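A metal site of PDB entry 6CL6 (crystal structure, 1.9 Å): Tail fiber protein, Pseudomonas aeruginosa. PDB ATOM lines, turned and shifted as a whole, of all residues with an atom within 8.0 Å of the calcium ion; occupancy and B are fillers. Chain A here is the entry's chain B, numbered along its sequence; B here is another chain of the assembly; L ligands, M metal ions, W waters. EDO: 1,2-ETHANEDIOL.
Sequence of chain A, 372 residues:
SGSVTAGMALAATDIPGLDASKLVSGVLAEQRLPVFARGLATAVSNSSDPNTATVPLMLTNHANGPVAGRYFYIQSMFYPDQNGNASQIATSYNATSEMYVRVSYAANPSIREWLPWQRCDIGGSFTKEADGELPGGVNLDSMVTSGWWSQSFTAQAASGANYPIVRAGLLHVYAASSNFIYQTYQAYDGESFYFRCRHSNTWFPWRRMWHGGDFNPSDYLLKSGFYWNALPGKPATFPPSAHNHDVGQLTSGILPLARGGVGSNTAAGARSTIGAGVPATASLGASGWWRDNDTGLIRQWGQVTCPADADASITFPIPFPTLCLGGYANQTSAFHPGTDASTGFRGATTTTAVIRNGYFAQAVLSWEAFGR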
ATOM      1  N   ALA A 308      -1.940 -14.808   2.827  1.00  0.00           N
ATOM      2  CA  ALA A 308      -0.558 -14.636   3.232  1.00  0.00           C
ATOM      3  C   ALA A 308      -0.130 -13.172   3.130  1.00  0.00           C
ATOM      4  O   ALA A 308      -0.364 -12.519   2.115  1.00  0.00           O
ATOM      5  CB  ALA A 308       0.325 -15.502   2.311  1.00  0.00           C
ATOM      6  N   ASP A 309       0.532 -12.683   4.174  1.00  0.00           N
ATOM      7  CA  ASP A 309       1.117 -11.341   4.168  1.00  0.00           C
ATOM      8  C   ASP A 309       0.162 -10.286   3.637  1.00  0.00           C
ATOM      9  O   ASP A 309       0.550  -9.432   2.828  1.00  0.00           O
ATOM     10  CB  ASP A 309       2.414 -11.304   3.347  1.00  0.00           C
ATOM     11  CG  ASP A 309       3.598 -11.968   4.042  1.00  0.00           C
ATOM     12  OD1 ASP A 309       3.689 -11.959   5.290  1.00  0.00           O
ATOM     13  OD2 ASP A 309       4.492 -12.493   3.311  1.00  0.00           O
ATOM     14  N   ALA A 310      -1.106 -10.318   4.081  1.00  0.00           N
ATOM     15  CA  ALA A 310      -2.113  -9.445   3.473  1.00  0.00           C
ATOM     16  C   ALA A 310      -3.334  -9.284   4.393  1.00  0.00           C
ATOM     17  O   ALA A 310      -3.429  -9.911   5.444  1.00  0.00           O
ATOM     18  CB  ALA A 310      -2.569  -9.983   2.123  1.00  0.00           C
ATOM     19  N   THR A 339       9.759 -17.139  11.720  1.00  0.00           N
ATOM     20  CA  THR A 339       9.369 -15.987  10.917  1.00  0.00           C
ATOM     21  C   THR A 339       8.337 -15.202  11.707  1.00  0.00           C
ATOM     22  O   THR A 339       7.798 -15.658  12.710  1.00  0.00           O
ATOM     23  CB  THR A 339       8.815 -16.408   9.538  1.00  0.00           C
ATOM     24  OG1 THR A 339       8.736 -15.258   8.687  1.00  0.00           O
ATOM     25  CG2 THR A 339       7.408 -16.988   9.697  1.00  0.00           C
ATOM     26  N   ASP A 340       8.051 -14.003  11.205  1.00  0.00           N
ATOM     27  CA  ASP A 340       7.034 -13.136  11.796  1.00  0.00           C
ATOM     28  C   ASP A 340       5.630 -13.669  11.525  1.00  0.00           C
ATOM     29  O   ASP A 340       5.329 -14.202  10.452  1.00  0.00           O
ATOM     30  CB  ASP A 340       7.151 -11.714  11.237  1.00  0.00           C
ATOM     31  CG  ASP A 340       7.273 -11.675   9.731  1.00  0.00           C
ATOM     32  OD1 ASP A 340       8.361 -12.045   9.225  1.00  0.00           O
ATOM     33  OD2 ASP A 340       6.291 -11.255   9.043  1.00  0.00           O
ATOM     34  N   ALA A 341       4.767 -13.518  12.528  1.00  0.00           N
ATOM     35  CA  ALA A 341       3.347 -13.891  12.397  1.00  0.00           C
ATOM     36  C   ALA A 341       2.514 -12.787  13.018  1.00  0.00           C
ATOM     37  O   ALA A 341       1.627 -13.033  13.843  1.00  0.00           O
ATOM     38  CB  ALA A 341       3.100 -15.252  13.041  1.00  0.00           C
ATOM     39  N   SER A 342       2.787 -11.547  12.628  1.00  0.00           N
ATOM     40  CA  SER A 342       2.155 -10.393  13.248  1.00  0.00           C
ATOM     41  C   SER A 342       0.695 -10.300  12.831  1.00  0.00           C
ATOM     42  O   SER A 342       0.224 -11.001  11.925  1.00  0.00           O
ATOM     43  CB  SER A 342       2.915  -9.116  12.922  1.00  0.00           C
ATOM     44  OG  SER A 342       4.217  -9.139  13.479  1.00  0.00           O
ATOM     45  N   ASN A 357      -2.627  -9.998   8.335  1.00  0.00           N
ATOM     46  CA  ASN A 357      -1.882 -11.209   8.669  1.00  0.00           C
ATOM     47  C   ASN A 357      -0.456 -11.060   8.161  1.00  0.00           C
ATOM     48  O   ASN A 357      -0.229 -11.034   6.957  1.00  0.00           O
ATOM     49  CB  ASN A 357      -2.541 -12.431   8.037  1.00  0.00           C
ATOM     50  CG  ASN A 357      -1.684 -13.668   8.139  1.00  0.00           C
ATOM     51  OD1 ASN A 357      -1.000 -13.881   9.114  1.00  0.00           O
ATOM     52  ND2 ASN A 357      -1.725 -14.499   7.075  1.00  0.00           N
ATOM     53  N   GLY A 358       0.508 -10.979   9.091  1.00  0.00           N
ATOM     54  CA  GLY A 358       1.911 -10.849   8.745  1.00  0.00           C
ATOM     55  C   GLY A 358       2.613 -12.175   8.468  1.00  0.00           C
ATOM     56  O   GLY A 358       3.733 -12.184   8.020  1.00  0.00           O
ATOM     57  N   TYR A 359       1.925 -13.300   8.719  1.00  0.00           N
ATOM     58  CA  TYR A 359       2.503 -14.619   8.469  1.00  0.00           C
ATOM     59  C   TYR A 359       2.625 -14.875   6.971  1.00  0.00           C
ATOM     60  O   TYR A 359       1.778 -14.427   6.170  1.00  0.00           O
ATOM     61  CB  TYR A 359       1.642 -15.704   9.109  1.00  0.00           C
ATOM     62  CG  TYR A 359       2.291 -17.070   9.175  1.00  0.00           C
ATOM     63  CD1 TYR A 359       3.523 -17.256   9.799  1.00  0.00           C
ATOM     64  CD2 TYR A 359       1.648 -18.193   8.645  1.00  0.00           C
ATOM     65  CE1 TYR A 359       4.109 -18.525   9.880  1.00  0.00           C
ATOM     66  CE2 TYR A 359       2.242 -19.464   8.719  1.00  0.00           C
ATOM     67  CZ  TYR A 359       3.448 -19.623   9.339  1.00  0.00           C
ATOM     68  OH  TYR A 359       4.001 -20.865   9.421  1.00  0.00           O
ATOM     69  N   PHE A 360       3.674 -15.607   6.595  1.00  0.00           N
ATOM     70  CA  PHE A 360       3.993 -15.784   5.192  1.00  0.00           C
ATOM     71  C   PHE A 360       3.018 -16.682   4.453  1.00  0.00           C
ATOM     72  O   PHE A 360       3.125 -16.784   3.219  1.00  0.00           O
ATOM     73  CB  PHE A 360       5.416 -16.365   5.060  1.00  0.00           C
ATOM     74  CG  PHE A 360       5.489 -17.836   5.298  1.00  0.00           C
ATOM     75  CD1 PHE A 360       5.606 -18.364   6.577  1.00  0.00           C
ATOM     76  CD2 PHE A 360       5.461 -18.718   4.231  1.00  0.00           C
ATOM     77  CE1 PHE A 360       5.665 -19.739   6.793  1.00  0.00           C
ATOM     78  CE2 PHE A 360       5.546 -20.075   4.426  1.00  0.00           C
ATOM     79  CZ  PHE A 360       5.638 -20.591   5.704  1.00  0.00           C
ATOM     80  N   ALA A 361       2.124 -17.350   5.155  1.00  0.00           N
ATOM     81  CA  ALA A 361       1.124 -18.229   4.535  1.00  0.00           C
ATOM     82  C   ALA A 361      -0.275 -17.819   4.974  1.00  0.00           C
ATOM     83  O   ALA A 361      -0.441 -17.102   5.955  1.00  0.00           O
ATOM     84  CB  ALA A 361       1.364 -19.696   4.896  1.00  0.00           C
ATOM     85  N   PHE B 335       1.234  -2.320   8.149  1.00  0.00           N
ATOM     86  CA  PHE B 335       2.663  -2.565   8.294  1.00  0.00           C
ATOM     87  C   PHE B 335       3.190  -3.498   7.204  1.00  0.00           C
ATOM     88  O   PHE B 335       2.521  -4.437   6.753  1.00  0.00           O
ATOM     89  CB  PHE B 335       2.953  -3.200   9.669  1.00  0.00           C
ATOM     90  CG  PHE B 335       2.207  -4.485   9.923  1.00  0.00           C
ATOM     91  CD1 PHE B 335       2.629  -5.687   9.383  1.00  0.00           C
ATOM     92  CD2 PHE B 335       1.102  -4.503  10.786  1.00  0.00           C
ATOM     93  CE1 PHE B 335       1.964  -6.861   9.640  1.00  0.00           C
ATOM     94  CE2 PHE B 335       0.428  -5.662  11.045  1.00  0.00           C
ATOM     95  CZ  PHE B 335       0.835  -6.850  10.485  1.00  0.00           C
ATOM     96  N   HIS B 336       4.420  -3.246   6.788  1.00  0.00           N
ATOM     97  CA  HIS B 336       5.048  -4.088   5.759  1.00  0.00           C
ATOM     98  C   HIS B 336       5.135  -5.519   6.246  1.00  0.00           C
ATOM     99  O   HIS B 336       5.757  -5.771   7.296  1.00  0.00           O
ATOM    100  CB  HIS B 336       6.422  -3.581   5.415  1.00  0.00           C
ATOM    101  CG  HIS B 336       6.963  -4.187   4.159  1.00  0.00           C
ATOM    102  ND1 HIS B 336       7.419  -5.485   4.102  1.00  0.00           N
ATOM    103  CD2 HIS B 336       7.094  -3.686   2.904  1.00  0.00           C
ATOM    104  CE1 HIS B 336       7.824  -5.750   2.874  1.00  0.00           C
ATOM    105  NE2 HIS B 336       7.642  -4.687   2.125  1.00  0.00           N
ATOM    106  N   PRO B 337       4.522  -6.485   5.545  1.00  0.00           N
ATOM    107  CA  PRO B 337       4.460  -7.863   6.066  1.00  0.00           C
ATOM    108  C   PRO B 337       5.728  -8.657   5.857  1.00  0.00           C
ATOM    109  O   PRO B 337       5.786  -9.840   6.239  1.00  0.00           O
ATOM    110  CB  PRO B 337       3.301  -8.474   5.267  1.00  0.00           C
ATOM    111  CG  PRO B 337       3.359  -7.760   3.974  1.00  0.00           C
ATOM    112  CD  PRO B 337       3.836  -6.354   4.255  1.00  0.00           C
ATOM    113  N   GLY B 338       6.772  -8.032   5.269  1.00  0.00           N
ATOM    114  CA  GLY B 338       8.079  -8.636   5.136  1.00  0.00           C
ATOM    115  C   GLY B 338       8.954  -8.560   6.360  1.00  0.00           C
ATOM    116  O   GLY B 338      10.067  -9.087   6.327  1.00  0.00           O
ATOM    117  N   THR B 339       8.491  -7.936   7.441  1.00  0.00           N
ATOM    118  CA  THR B 339       9.262  -7.780   8.655  1.00  0.00           C
ATOM    119  C   THR B 339       8.370  -8.047   9.872  1.00  0.00           C
ATOM    120  O   THR B 339       7.172  -8.218   9.746  1.00  0.00           O
ATOM    121  CB  THR B 339       9.901  -6.380   8.709  1.00  0.00           C
ATOM    122  OG1 THR B 339      10.855  -6.326   9.771  1.00  0.00           O
ATOM    123  CG2 THR B 339       8.846  -5.310   8.955  1.00  0.00           C
ATOM    124  N   ASP B 340       8.998  -8.080  11.060  1.00  0.00           N
ATOM    125  CA  ASP B 340       8.241  -8.254  12.285  1.00  0.00           C
ATOM    126  C   ASP B 340       7.429  -6.985  12.619  1.00  0.00           C
ATOM    127  O   ASP B 340       7.870  -5.843  12.378  1.00  0.00           O
ATOM    128  CB  ASP B 340       9.139  -8.596  13.467  1.00  0.00           C
ATOM    129  CG  ASP B 340       8.375  -8.608  14.813  1.00  0.00           C
ATOM    130  OD1 ASP B 340       7.707  -9.630  15.108  1.00  0.00           O
ATOM    131  OD2 ASP B 340       8.426  -7.602  15.576  1.00  0.00           O
ATOM    132  N   ALA B 341       6.247  -7.184  13.152  1.00  0.00           N
ATOM    133  CA  ALA B 341       5.408  -6.069  13.642  1.00  0.00           C
ATOM    134  C   ALA B 341       4.800  -6.472  14.979  1.00  0.00           C
ATOM    135  O   ALA B 341       3.620  -6.279  15.243  1.00  0.00           O
ATOM    136  CB  ALA B 341       4.354  -5.679  12.625  1.00  0.00           C
HETATM  137  C1  EDO L   1       7.755 -12.912   4.716  1.00  0.00           C
HETATM  138  O1  EDO L   1       6.343 -13.054   4.829  1.00  0.00           O
HETATM  139  C2  EDO L   1       8.431 -12.842   6.085  1.00  0.00           C
HETATM  140  O2  EDO L   1       7.981 -11.699   6.849  1.00  0.00           O
HETATM  141 CA    CA M   1       5.610 -12.025   6.863  1.00  0.00          CA
HETATM  142  O   HOH W   1       6.125 -14.251   7.901  1.00  0.00           O
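The backbone NH (N) of Gly 358 sits at hydrogen-bond distance from the backbone carbonyl oxygen (O) of Ser 342 (2.8 Å).
The backbone NH (N) of Asp 309 lies close to the backbone carbonyl oxygen (O) of Asn 357, 3.3 Å away.
The side-chain hydroxyl of Thr 339 of chain A lies within hydrogen-bond range of the side-chain carboxylate of Asp 340 of chain A (3.3 Å).
The backbone NH (N) of Asp 309 is in hydrogen-bond range of the backbone carbonyl oxygen (O) of Tyr 359.
Water W1 lies within hydrogen-bond range of the backbone carbonyl oxygen (O) of Asp 340 of chain A (2.7 Å), the side-chain hydroxyl (OG1) of Thr 339 of chain A (2.9 Å) and the backbone NH (N) of Phe 360 (3.1 Å).
The calcium ion is bound by O of Gly 358 (2.2 Å), O of Pro 337 of chain B (2.3 Å), O2 of the ligand (2.4 Å), O1 of the ligand (2.4 Å), OD2 of Asp 340 of chain A (2.4 Å), OD1 of Asp 309 (2.5 Å) and water W1 (2.5 Å).
The calcium ion has seven donor atoms within binding distance.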
